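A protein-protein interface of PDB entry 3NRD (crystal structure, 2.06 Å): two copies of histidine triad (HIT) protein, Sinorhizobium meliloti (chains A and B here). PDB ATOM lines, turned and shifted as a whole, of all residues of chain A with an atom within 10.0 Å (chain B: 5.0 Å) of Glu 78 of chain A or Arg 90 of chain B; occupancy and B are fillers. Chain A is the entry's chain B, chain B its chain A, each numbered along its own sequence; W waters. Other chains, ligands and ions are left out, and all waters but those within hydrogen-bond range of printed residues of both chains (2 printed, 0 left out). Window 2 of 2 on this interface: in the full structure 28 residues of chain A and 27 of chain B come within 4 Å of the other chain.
O of Lys 72 of chain A is in hydrogen-bond range of N of Ala 77 of chain A (3.3 Å). O of Glu 78 of chain A is in hydrogen-bond range of NZ of Lys 72 of chain A (3.4 Å). The backbone NH of Glu 101 of chain A sits at hydrogen-bond distance from the side-chain carboxylate of Glu 78 of chain A (2.9 Å). O of Lys 79 of chain A is in hydrogen-bond range of N of Arg 99 of chain A (2.7 Å). The backbone NH (N) of Asn 81 of chain A sits at hydrogen-bond distance from the backbone carbonyl oxygen (O) of Ile 97 of chain A. The side-chain amide oxygen (OD1) of Asn 81 of chain A lies within hydrogen-bond range of the guanidinium group (NH1) of Arg 99 of chain A, 3.1 Å away.
O of Lys 47 of chain B sits close to NZ of Lys 79 of chain A, 3.5 Å away. OE2 of Glu 48 of chain B lies within salt-bridge range of NZ of Lys 72 of chain A, at 3.1 Å. OE1 of Glu 48 of chain B lies within salt-bridge range of NZ of Lys 79 of chain A (2.6 Å). N of Ile 80 of chain A sits at hydrogen-bond distance from OE2 of Glu 48 of chain B (3.0 Å). ND2 of Asn 81 of chain A sits at hydrogen-bond distance from OD1 of Asn 87 of chain B (2.9 Å). ND2 of Asn 87 of chain B lies close to NH1 of Arg 99 of chain A, 3.2 Å away. The side-chain amide nitrogen (ND2) of Asn 87 of chain B sits at hydrogen-bond distance from the backbone carbonyl oxygen (O) of Pro 107 of chain A (2.9 Å). The side-chain carboxylate (OE2) of Glu 78 of chain A lies within salt-bridge range of the guanidinium group (NH2) of Arg 90 of chain B (2.7 Å).
Thr 75 of chain A touches none of the printed residues of chain B. Printed residues of chain B within 4 Å of Lys 79 of chain A: Lys 47 (3.4 Å), Glu 48 (2.6 Å), Gly 86 (3.7 Å), Asn 87 (3.5 Å) and Arg 90 (3.9 Å). Printed residues of chain B within 4 Å of Arg 99 of chain A: Asn 87 (3.2 Å). Arg 100 of chain A touches none of the printed residues of chain B. Printed residues of chain B within 4 Å of Trp 106 of chain A: Asn 87 and Arg 90. Of the printed residues of chain A, Glu 48 of chain B touches Lys 72 (3.1 Å), Lys 79 (2.6 Å) and Ile 80 (3.0 Å). No residue of chain A comes within 4 Å of Val 89 of chain B. Printed residues of chain A within 4 Å of Arg 90 of chain B: Glu 78 (2.7 Å), Lys 79 (3.9 Å) and Trp 106 (3.5 Å). The nearest printed residue of chain A that does not touch Arg 90 of chain B is Glu 101 of chain A (6.2 Å).
Lys 72 of chain A touches Lys 47 of chain B (NZ to CE, 3.9 Å). O of Glu 78 of chain A touches CE of Lys 47 of chain B (3.6 Å). Gly 86 of chain B touches Lys 79 of chain A. Asn 87 of chain B touches Lys 79 of chain A (OD1 to CG, 3.5 Å). Arg 90 of chain B touches Lys 79 of chain A (CD to CD, 3.9 Å). CZ3 of Trp 106 of chain A touches CG of Asn 87 of chain B (3.6 Å). Arg 90 of chain B touches Trp 106 of chain A (NH2 to CH2, 3.5 Å).
No position is printed for both chains. Of the 15 pairs that touch across the chains among the printed residues, none has its exchanged pair printed and touching as well.
Water W2 lies within hydrogen-bond range of the backbone carbonyl oxygen (O) of Pro 107 of chain A (2.6 Å) and the side-chain amide nitrogen (ND2) of Asn 87 of chain B (3.4 Å). Water W1 bridges NZ of Lys 79 of chain A (2.7 Å) and O of Lys 47 of chain B (2.9 Å).
Of the 22 printed residues of chain A, 8 touch a printed residue of chain B. Hydrophobic or aromatic side chains of chain A that line the printed part of chain B: Ile 80, Trp 106 and Pro 107.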
ATOM      1  N   PRO A  35     -35.634  15.337  14.799  1.00  0.00           N
ATOM      2  CA  PRO A  35     -35.952  16.489  15.656  1.00  0.00           C
ATOM      3  C   PRO A  35     -36.175  17.749  14.794  1.00  0.00           C
ATOM      4  O   PRO A  35     -35.243  18.242  14.176  1.00  0.00           O
ATOM      5  CB  PRO A  35     -34.720  16.609  16.553  1.00  0.00           C
ATOM      6  CG  PRO A  35     -34.168  15.284  16.608  1.00  0.00           C
ATOM      7  CD  PRO A  35     -34.417  14.661  15.259  1.00  0.00           C
ATOM      8  N   ALA A  68     -30.840  26.851  15.674  1.00  0.00           N
ATOM      9  CA  ALA A  68     -30.042  25.869  14.980  1.00  0.00           C
ATOM     10  C   ALA A  68     -28.876  25.444  15.849  1.00  0.00           C
ATOM     11  O   ALA A  68     -28.633  24.252  15.988  1.00  0.00           O
ATOM     12  CB  ALA A  68     -29.555  26.416  13.621  1.00  0.00           C
ATOM     13  N   LEU A  71     -30.533  23.550  18.900  1.00  0.00           N
ATOM     14  CA  LEU A  71     -30.996  22.218  18.469  1.00  0.00           C
ATOM     15  C   LEU A  71     -29.834  21.231  18.238  1.00  0.00           C
ATOM     16  O   LEU A  71     -29.939  20.055  18.645  1.00  0.00           O
ATOM     17  CB  LEU A  71     -31.872  22.331  17.207  1.00  0.00           C
ATOM     18  CG  LEU A  71     -32.529  21.058  16.634  1.00  0.00           C
ATOM     19  CD1 LEU A  71     -33.456  20.381  17.626  1.00  0.00           C
ATOM     20  CD2 LEU A  71     -33.279  21.405  15.343  1.00  0.00           C
ATOM     21  N   LYS A  72     -28.733  21.696  17.612  1.00  0.00           N
ATOM     22  CA  LYS A  72     -27.541  20.823  17.443  1.00  0.00           C
ATOM     23  C   LYS A  72     -27.006  20.315  18.791  1.00  0.00           C
ATOM     24  O   LYS A  72     -26.721  19.115  18.944  1.00  0.00           O
ATOM     25  CB  LYS A  72     -26.414  21.526  16.639  1.00  0.00           C
ATOM     26  CG  LYS A  72     -25.242  20.608  16.183  1.00  0.00           C
ATOM     27  CD  LYS A  72     -24.361  21.298  15.084  1.00  0.00           C
ATOM     28  CE  LYS A  72     -23.126  20.472  14.645  1.00  0.00           C
ATOM     29  NZ  LYS A  72     -22.802  20.654  13.162  1.00  0.00           N
ATOM     30  N   LYS A  73     -26.876  21.231  19.753  1.00  0.00           N
ATOM     31  CA  LYS A  73     -26.429  20.892  21.095  1.00  0.00           C
ATOM     32  C   LYS A  73     -27.396  19.909  21.740  1.00  0.00           C
ATOM     33  O   LYS A  73     -26.973  18.950  22.373  1.00  0.00           O
ATOM     34  CB  LYS A  73     -26.340  22.128  22.002  1.00  0.00           C
ATOM     35  CG  LYS A  73     -25.087  22.959  21.926  1.00  0.00           C
ATOM     36  CD  LYS A  73     -24.728  23.547  23.340  1.00  0.00           C
ATOM     37  N   ALA A  74     -28.688  20.175  21.607  1.00  0.00           N
ATOM     38  CA  ALA A  74     -29.714  19.362  22.252  1.00  0.00           C
ATOM     39  C   ALA A  74     -29.745  17.924  21.733  1.00  0.00           C
ATOM     40  O   ALA A  74     -30.083  17.013  22.503  1.00  0.00           O
ATOM     41  CB  ALA A  74     -31.056  19.989  22.073  1.00  0.00           C
ATOM     42  N   THR A  75     -29.418  17.742  20.448  1.00  0.00           N
ATOM     43  CA  THR A  75     -29.634  16.484  19.734  1.00  0.00           C
ATOM     44  C   THR A  75     -28.360  15.756  19.342  1.00  0.00           C
ATOM     45  O   THR A  75     -28.433  14.629  18.937  1.00  0.00           O
ATOM     46  CB  THR A  75     -30.414  16.738  18.423  1.00  0.00           C
ATOM     47  OG1 THR A  75     -29.606  17.534  17.541  1.00  0.00           O
ATOM     48  CG2 THR A  75     -31.764  17.447  18.711  1.00  0.00           C
ATOM     49  N   GLY A  76     -27.196  16.366  19.494  1.00  0.00           N
ATOM     50  CA  GLY A  76     -25.952  15.838  18.919  1.00  0.00           C
ATOM     51  C   GLY A  76     -25.997  15.705  17.405  1.00  0.00           C
ATOM     52  O   GLY A  76     -25.454  14.782  16.856  1.00  0.00           O
ATOM     53  N   ALA A  77     -26.670  16.623  16.734  1.00  0.00           N
ATOM     54  CA  ALA A  77     -26.928  16.469  15.302  1.00  0.00           C
ATOM     55  C   ALA A  77     -25.602  16.556  14.587  1.00  0.00           C
ATOM     56  O   ALA A  77     -24.706  17.269  15.048  1.00  0.00           O
ATOM     57  CB  ALA A  77     -27.885  17.535  14.794  1.00  0.00           C
ATOM     58  N   GLU A  78     -25.444  15.761  13.525  1.00  0.00           N
ATOM     59  CA  GLU A  78     -24.321  15.888  12.594  1.00  0.00           C
ATOM     60  C   GLU A  78     -24.475  17.166  11.759  1.00  0.00           C
ATOM     61  O   GLU A  78     -23.504  17.851  11.419  1.00  0.00           O
ATOM     62  CB  GLU A  78     -24.283  14.659  11.683  1.00  0.00           C
ATOM     63  CG  GLU A  78     -23.189  14.651  10.655  1.00  0.00           C
ATOM     64  CD  GLU A  78     -23.135  13.386   9.797  1.00  0.00           C
ATOM     65  OE1 GLU A  78     -23.860  12.407  10.106  1.00  0.00           O
ATOM     66  OE2 GLU A  78     -22.364  13.422   8.796  1.00  0.00           O
ATOM     67  N   LYS A  79     -25.715  17.468  11.406  1.00  0.00           N
ATOM     68  CA  LYS A  79     -26.001  18.609  10.563  1.00  0.00           C
ATOM     69  C   LYS A  79     -27.376  19.150  10.844  1.00  0.00           C
ATOM     70  O   LYS A  79     -28.316  18.396  11.120  1.00  0.00           O
ATOM     71  CB  LYS A  79     -25.883  18.209   9.076  1.00  0.00           C
ATOM     72  CG  LYS A  79     -25.868  19.359   8.052  1.00  0.00           C
ATOM     73  CD  LYS A  79     -24.590  20.220   8.120  1.00  0.00           C
ATOM     74  CE  LYS A  79     -24.666  21.533   7.286  1.00  0.00           C
ATOM     75  NZ  LYS A  79     -25.816  22.389   7.631  1.00  0.00           N
ATOM     76  N   ILE A  80     -27.490  20.469  10.782  1.00  0.00           N
ATOM     77  CA  ILE A  80     -28.760  21.151  10.865  1.00  0.00           C
ATOM     78  C   ILE A  80     -29.210  21.524   9.459  1.00  0.00           C
ATOM     79  O   ILE A  80     -28.403  22.024   8.662  1.00  0.00           O
ATOM     80  CB  ILE A  80     -28.699  22.447  11.684  1.00  0.00           C
ATOM     81  CG1 ILE A  80     -28.267  22.187  13.122  1.00  0.00           C
ATOM     82  CG2 ILE A  80     -30.065  23.099  11.709  1.00  0.00           C
ATOM     83  CD1 ILE A  80     -29.185  21.312  13.922  1.00  0.00           C
ATOM     84  N   ASN A  81     -30.488  21.283   9.163  1.00  0.00           N
ATOM     85  CA  ASN A  81     -31.101  21.731   7.914  1.00  0.00           C
ATOM     86  C   ASN A  81     -32.097  22.846   8.192  1.00  0.00           C
ATOM     87  O   ASN A  81     -32.941  22.727   9.090  1.00  0.00           O
ATOM     88  CB  ASN A  81     -31.838  20.596   7.197  1.00  0.00           C
ATOM     89  CG  ASN A  81     -30.901  19.493   6.654  1.00  0.00           C
ATOM     90  OD1 ASN A  81     -31.387  18.485   6.109  1.00  0.00           O
ATOM     91  ND2 ASN A  81     -29.587  19.680   6.774  1.00  0.00           N
ATOM     92  N   ILE A  97     -34.076  21.713  11.501  1.00  0.00           N
ATOM     93  CA  ILE A  97     -34.146  20.270  11.613  1.00  0.00           C
ATOM     94  C   ILE A  97     -32.763  19.664  11.927  1.00  0.00           C
ATOM     95  O   ILE A  97     -31.762  19.971  11.252  1.00  0.00           O
ATOM     96  CB  ILE A  97     -34.682  19.648  10.317  1.00  0.00           C
ATOM     97  CG1 ILE A  97     -36.091  20.148   9.972  1.00  0.00           C
ATOM     98  CG2 ILE A  97     -34.719  18.112  10.436  1.00  0.00           C
ATOM     99  CD1 ILE A  97     -36.427  20.036   8.517  1.00  0.00           C
ATOM    100  N   ALA A  98     -32.718  18.792  12.933  1.00  0.00           N
ATOM    101  CA  ALA A  98     -31.509  18.065  13.322  1.00  0.00           C
ATOM    102  C   ALA A  98     -31.383  16.848  12.453  1.00  0.00           C
ATOM    103  O   ALA A  98     -32.322  16.037  12.394  1.00  0.00           O
ATOM    104  CB  ALA A  98     -31.613  17.656  14.762  1.00  0.00           C
ATOM    105  N   ARG A  99     -30.259  16.710  11.764  1.00  0.00           N
ATOM    106  CA  ARG A  99     -29.986  15.548  10.913  1.00  0.00           C
ATOM    107  C   ARG A  99     -28.734  14.810  11.327  1.00  0.00           C
ATOM    108  O   ARG A  99     -27.806  15.385  11.941  1.00  0.00           O
ATOM    109  CB  ARG A  99     -29.812  15.957   9.453  1.00  0.00           C
ATOM    110  CG  ARG A  99     -30.968  16.739   8.852  1.00  0.00           C
ATOM    111  CD  ARG A  99     -32.278  15.980   8.896  1.00  0.00           C
ATOM    112  NE  ARG A  99     -32.237  14.721   8.152  1.00  0.00           N
ATOM    113  CZ  ARG A  99     -32.414  14.586   6.832  1.00  0.00           C
ATOM    114  NH1 ARG A  99     -32.609  15.634   6.020  1.00  0.00           N
ATOM    115  NH2 ARG A  99     -32.370  13.363   6.288  1.00  0.00           N
ATOM    116  N   ARG A 100     -28.725  13.528  10.980  1.00  0.00           N
ATOM    117  CA  ARG A 100     -27.537  12.700  11.095  1.00  0.00           C
ATOM    118  C   ARG A 100     -27.598  11.507  10.118  1.00  0.00           C
ATOM    119  O   ARG A 100     -28.676  11.048   9.713  1.00  0.00           O
ATOM    120  CB  ARG A 100     -27.260  12.338  12.589  1.00  0.00           C
ATOM    121  CG  ARG A 100     -27.671  10.984  13.114  1.00  0.00           C
ATOM    122  CD  ARG A 100     -28.422  11.076  14.425  1.00  0.00           C
ATOM    123  NE  ARG A 100     -27.605  11.319  15.621  1.00  0.00           N
ATOM    124  CZ  ARG A 100     -27.738  12.328  16.503  1.00  0.00           C
ATOM    125  NH1 ARG A 100     -28.630  13.335  16.356  1.00  0.00           N
ATOM    126  NH2 ARG A 100     -26.935  12.336  17.578  1.00  0.00           N
ATOM    127  N   GLU A 101     -26.423  11.075   9.669  1.00  0.00           N
ATOM    128  CA  GLU A 101     -26.311   9.884   8.857  1.00  0.00           C
ATOM    129  C   GLU A 101     -27.087   8.727   9.482  1.00  0.00           C
ATOM    130  O   GLU A 101     -27.049   8.524  10.691  1.00  0.00           O
ATOM    131  CB  GLU A 101     -24.844   9.509   8.699  1.00  0.00           C
ATOM    132  CG  GLU A 101     -24.624   8.217   8.003  1.00  0.00           C
ATOM    133  CD  GLU A 101     -23.204   8.089   7.536  1.00  0.00           C
ATOM    134  OE1 GLU A 101     -22.317   7.939   8.406  1.00  0.00           O
ATOM    135  OE2 GLU A 101     -22.992   8.141   6.306  1.00  0.00           O
ATOM    136  N   GLY A 102     -27.801   7.984   8.652  1.00  0.00           N
ATOM    137  CA  GLY A 102     -28.663   6.918   9.154  1.00  0.00           C
ATOM    138  C   GLY A 102     -30.086   7.339   9.467  1.00  0.00           C
ATOM    139  O   GLY A 102     -30.946   6.483   9.556  1.00  0.00           O
ATOM    140  N   ASP A 103     -30.377   8.630   9.616  1.00  0.00           N
ATOM    141  CA  ASP A 103     -31.743   9.030   9.925  1.00  0.00           C
ATOM    142  C   ASP A 103     -32.648   8.856   8.676  1.00  0.00           C
ATOM    143  O   ASP A 103     -32.142   8.680   7.558  1.00  0.00           O
ATOM    144  CB  ASP A 103     -31.818  10.447  10.544  1.00  0.00           C
ATOM    145  CG  ASP A 103     -31.706  11.564   9.531  1.00  0.00           C
ATOM    146  OD1 ASP A 103     -31.890  11.373   8.312  1.00  0.00           O
ATOM    147  OD2 ASP A 103     -31.403  12.692   9.974  1.00  0.00           O
ATOM    148  N   TRP A 106     -31.956   9.985   4.961  1.00  0.00           N
ATOM    149  CA  TRP A 106     -30.639  10.590   4.874  1.00  0.00           C
ATOM    150  C   TRP A 106     -29.974  10.166   3.556  1.00  0.00           C
ATOM    151  O   TRP A 106     -30.008   9.003   3.237  1.00  0.00           O
ATOM    152  CB  TRP A 106     -29.731  10.164   6.027  1.00  0.00           C
ATOM    153  CG  TRP A 106     -28.317  10.641   5.833  1.00  0.00           C
ATOM    154  CD1 TRP A 106     -27.324  10.008   5.153  1.00  0.00           C
ATOM    155  CD2 TRP A 106     -27.754  11.857   6.315  1.00  0.00           C
ATOM    156  NE1 TRP A 106     -26.166  10.751   5.185  1.00  0.00           N
ATOM    157  CE2 TRP A 106     -26.402  11.890   5.904  1.00  0.00           C
ATOM    158  CE3 TRP A 106     -28.247  12.907   7.085  1.00  0.00           C
ATOM    159  CZ2 TRP A 106     -25.549  12.942   6.223  1.00  0.00           C
ATOM    160  CZ3 TRP A 106     -27.397  13.952   7.408  1.00  0.00           C
ATOM    161  CH2 TRP A 106     -26.070  13.968   6.963  1.00  0.00           C
ATOM    162  N   PRO A 107     -29.344  11.089   2.816  1.00  0.00           N
ATOM    163  CA  PRO A 107     -29.081  12.509   3.065  1.00  0.00           C
ATOM    164  C   PRO A 107     -30.118  13.452   2.500  1.00  0.00           C
ATOM    165  O   PRO A 107     -29.938  14.656   2.627  1.00  0.00           O
ATOM    166  CB  PRO A 107     -27.752  12.744   2.339  1.00  0.00           C
ATOM    167  CG  PRO A 107     -27.860  11.845   1.125  1.00  0.00           C
ATOM    168  CD  PRO A 107     -28.697  10.641   1.562  1.00  0.00           C
ATOM    169  N   ARG B  10     -17.940  19.755  -5.852  1.00  0.00           N
ATOM    170  CA  ARG B  10     -19.256  19.290  -6.283  1.00  0.00           C
ATOM    171  C   ARG B  10     -20.171  20.465  -6.597  1.00  0.00           C
ATOM    172  O   ARG B  10     -20.990  20.362  -7.528  1.00  0.00           O
ATOM    173  CB  ARG B  10     -19.883  18.350  -5.274  1.00  0.00           C
ATOM    174  CG  ARG B  10     -19.133  17.004  -5.196  1.00  0.00           C
ATOM    175  CD  ARG B  10     -19.279  16.369  -3.860  1.00  0.00           C
ATOM    176  NE  ARG B  10     -18.652  17.183  -2.811  1.00  0.00           N
ATOM    177  CZ  ARG B  10     -18.738  16.932  -1.509  1.00  0.00           C
ATOM    178  NH1 ARG B  10     -19.408  15.868  -1.052  1.00  0.00           N
ATOM    179  NH2 ARG B  10     -18.137  17.742  -0.653  1.00  0.00           N
ATOM    180  N   ILE B  46     -16.855  26.812   6.682  1.00  0.00           N
ATOM    181  CA  ILE B  46     -18.139  27.120   7.303  1.00  0.00           C
ATOM    182  C   ILE B  46     -19.134  26.060   6.845  1.00  0.00           C
ATOM    183  O   ILE B  46     -19.293  25.842   5.640  1.00  0.00           O
ATOM    184  CB  ILE B  46     -18.659  28.552   6.940  1.00  0.00           C
ATOM    185  CG1 ILE B  46     -17.684  29.653   7.422  1.00  0.00           C
ATOM    186  CG2 ILE B  46     -20.116  28.790   7.471  1.00  0.00           C
ATOM    187  CD1 ILE B  46     -17.345  29.666   8.932  1.00  0.00           C
ATOM    188  N   LYS B  47     -19.792  25.415   7.817  1.00  0.00           N
ATOM    189  CA  LYS B  47     -20.793  24.369   7.531  1.00  0.00           C
ATOM    190  C   LYS B  47     -22.201  24.779   7.968  1.00  0.00           C
ATOM    191  O   LYS B  47     -23.156  24.597   7.207  1.00  0.00           O
ATOM    192  CB  LYS B  47     -20.353  23.001   8.110  1.00  0.00           C
ATOM    193  CG  LYS B  47     -20.955  22.566   9.427  1.00  0.00           C
ATOM    194  CD  LYS B  47     -20.350  21.245   9.941  1.00  0.00           C
ATOM    195  CE  LYS B  47     -21.254  20.059   9.660  1.00  0.00           C
ATOM    196  N   GLU B  48     -22.344  25.369   9.151  1.00  0.00           N
ATOM    197  CA  GLU B  48     -23.639  25.841   9.607  1.00  0.00           C
ATOM    198  C   GLU B  48     -23.691  27.340   9.488  1.00  0.00           C
ATOM    199  O   GLU B  48     -22.676  28.011   9.716  1.00  0.00           O
ATOM    200  CB  GLU B  48     -23.914  25.442  11.065  1.00  0.00           C
ATOM    201  CG  GLU B  48     -23.760  23.955  11.436  1.00  0.00           C
ATOM    202  CD  GLU B  48     -24.823  23.019  10.821  1.00  0.00           C
ATOM    203  OE1 GLU B  48     -25.635  23.475  10.012  1.00  0.00           O
ATOM    204  OE2 GLU B  48     -24.810  21.808  11.142  1.00  0.00           O
ATOM    205  N   GLY B  86     -26.930  20.946   3.302  1.00  0.00           N
ATOM    206  CA  GLY B  86     -25.572  20.541   3.456  1.00  0.00           C
ATOM    207  C   GLY B  86     -25.341  19.168   4.014  1.00  0.00           C
ATOM    208  O   GLY B  86     -24.309  18.941   4.643  1.00  0.00           O
ATOM    209  N   ASN B  87     -26.262  18.247   3.773  1.00  0.00           N
ATOM    210  CA  ASN B  87     -26.034  16.865   4.158  1.00  0.00           C
ATOM    211  C   ASN B  87     -25.022  16.274   3.158  1.00  0.00           C
ATOM    212  O   ASN B  87     -24.196  15.483   3.552  1.00  0.00           O
ATOM    213  CB  ASN B  87     -27.333  16.034   4.218  1.00  0.00           C
ATOM    214  CG  ASN B  87     -28.391  16.627   5.180  1.00  0.00           C
ATOM    215  OD1 ASN B  87     -28.050  17.296   6.161  1.00  0.00           O
ATOM    216  ND2 ASN B  87     -29.677  16.399   4.879  1.00  0.00           N
ATOM    217  N   ILE B  88     -25.073  16.746   1.901  1.00  0.00           N
ATOM    218  CA  ILE B  88     -24.261  16.249   0.778  1.00  0.00           C
ATOM    219  C   ILE B  88     -22.907  17.023   0.807  1.00  0.00           C
ATOM    220  O   ILE B  88     -21.877  16.523   1.257  1.00  0.00           O
ATOM    221  CB  ILE B  88     -25.137  16.317  -0.580  1.00  0.00           C
ATOM    222  CG1 ILE B  88     -26.419  15.453  -0.450  1.00  0.00           C
ATOM    223  CG2 ILE B  88     -24.369  15.896  -1.835  1.00  0.00           C
ATOM    224  CD1 ILE B  88     -27.418  15.518  -1.673  1.00  0.00           C
ATOM    225  N   VAL B  89     -22.969  18.286   0.424  1.00  0.00           N
ATOM    226  CA  VAL B  89     -21.833  19.179   0.416  1.00  0.00           C
ATOM    227  C   VAL B  89     -21.852  19.989   1.683  1.00  0.00           C
ATOM    228  O   VAL B  89     -22.781  20.769   1.901  1.00  0.00           O
ATOM    229  CB  VAL B  89     -21.966  20.119  -0.783  1.00  0.00           C
ATOM    230  CG1 VAL B  89     -20.898  21.231  -0.770  1.00  0.00           C
ATOM    231  CG2 VAL B  89     -21.934  19.291  -2.031  1.00  0.00           C
ATOM    232  N   ARG B  90     -20.826  19.842   2.511  1.00  0.00           N
ATOM    233  CA  ARG B  90     -20.791  20.512   3.830  1.00  0.00           C
ATOM    234  C   ARG B  90     -20.472  21.992   3.817  1.00  0.00           C
ATOM    235  O   ARG B  90     -20.901  22.693   4.710  1.00  0.00           O
ATOM    236  CB  ARG B  90     -19.786  19.831   4.773  1.00  0.00           C
ATOM    237  CG  ARG B  90     -20.296  18.535   5.315  1.00  0.00           C
ATOM    238  CD  ARG B  90     -21.473  18.750   6.271  1.00  0.00           C
ATOM    239  NE  ARG B  90     -22.286  17.541   6.346  1.00  0.00           N
ATOM    240  CZ  ARG B  90     -22.227  16.637   7.319  1.00  0.00           C
ATOM    241  NH1 ARG B  90     -21.425  16.776   8.389  1.00  0.00           N
ATOM    242  NH2 ARG B  90     -23.009  15.575   7.219  1.00  0.00           N
ATOM    243  N   GLN B  91     -19.694  22.447   2.852  1.00  0.00           N
ATOM    244  CA  GLN B  91     -19.484  23.857   2.641  1.00  0.00           C
ATOM    245  C   GLN B  91     -20.835  24.595   2.551  1.00  0.00           C
ATOM    246  O   GLN B  91     -21.710  24.197   1.780  1.00  0.00           O
ATOM    247  CB  GLN B  91     -18.703  24.064   1.354  1.00  0.00           C
ATOM    248  CG  GLN B  91     -18.391  25.505   1.050  1.00  0.00           C
ATOM    249  CD  GLN B  91     -17.455  25.632  -0.105  1.00  0.00           C
ATOM    250  OE1 GLN B  91     -17.852  25.447  -1.254  1.00  0.00           O
ATOM    251  NE2 GLN B  91     -16.203  25.907   0.182  1.00  0.00           N
ATOM    252  N   LEU B  92     -20.982  25.629   3.383  1.00  0.00           N
ATOM    253  CA  LEU B  92     -22.222  26.355   3.520  1.00  0.00           C
ATOM    254  C   LEU B  92     -22.654  26.890   2.147  1.00  0.00           C
ATOM    255  O   LEU B  92     -21.890  27.555   1.485  1.00  0.00           O
ATOM    256  CB  LEU B  92     -22.082  27.528   4.519  1.00  0.00           C
ATOM    257  CG  LEU B  92     -23.321  28.473   4.655  1.00  0.00           C
ATOM    258  CD1 LEU B  92     -24.643  27.707   5.002  1.00  0.00           C
ATOM    259  CD2 LEU B  92     -23.046  29.558   5.688  1.00  0.00           C
HETATM  260  O   HOH W   1     -25.846  24.674   6.249  1.00  0.00           O
HETATM  261  O   HOH W   2     -31.052  16.861   1.811  1.00  0.00           O
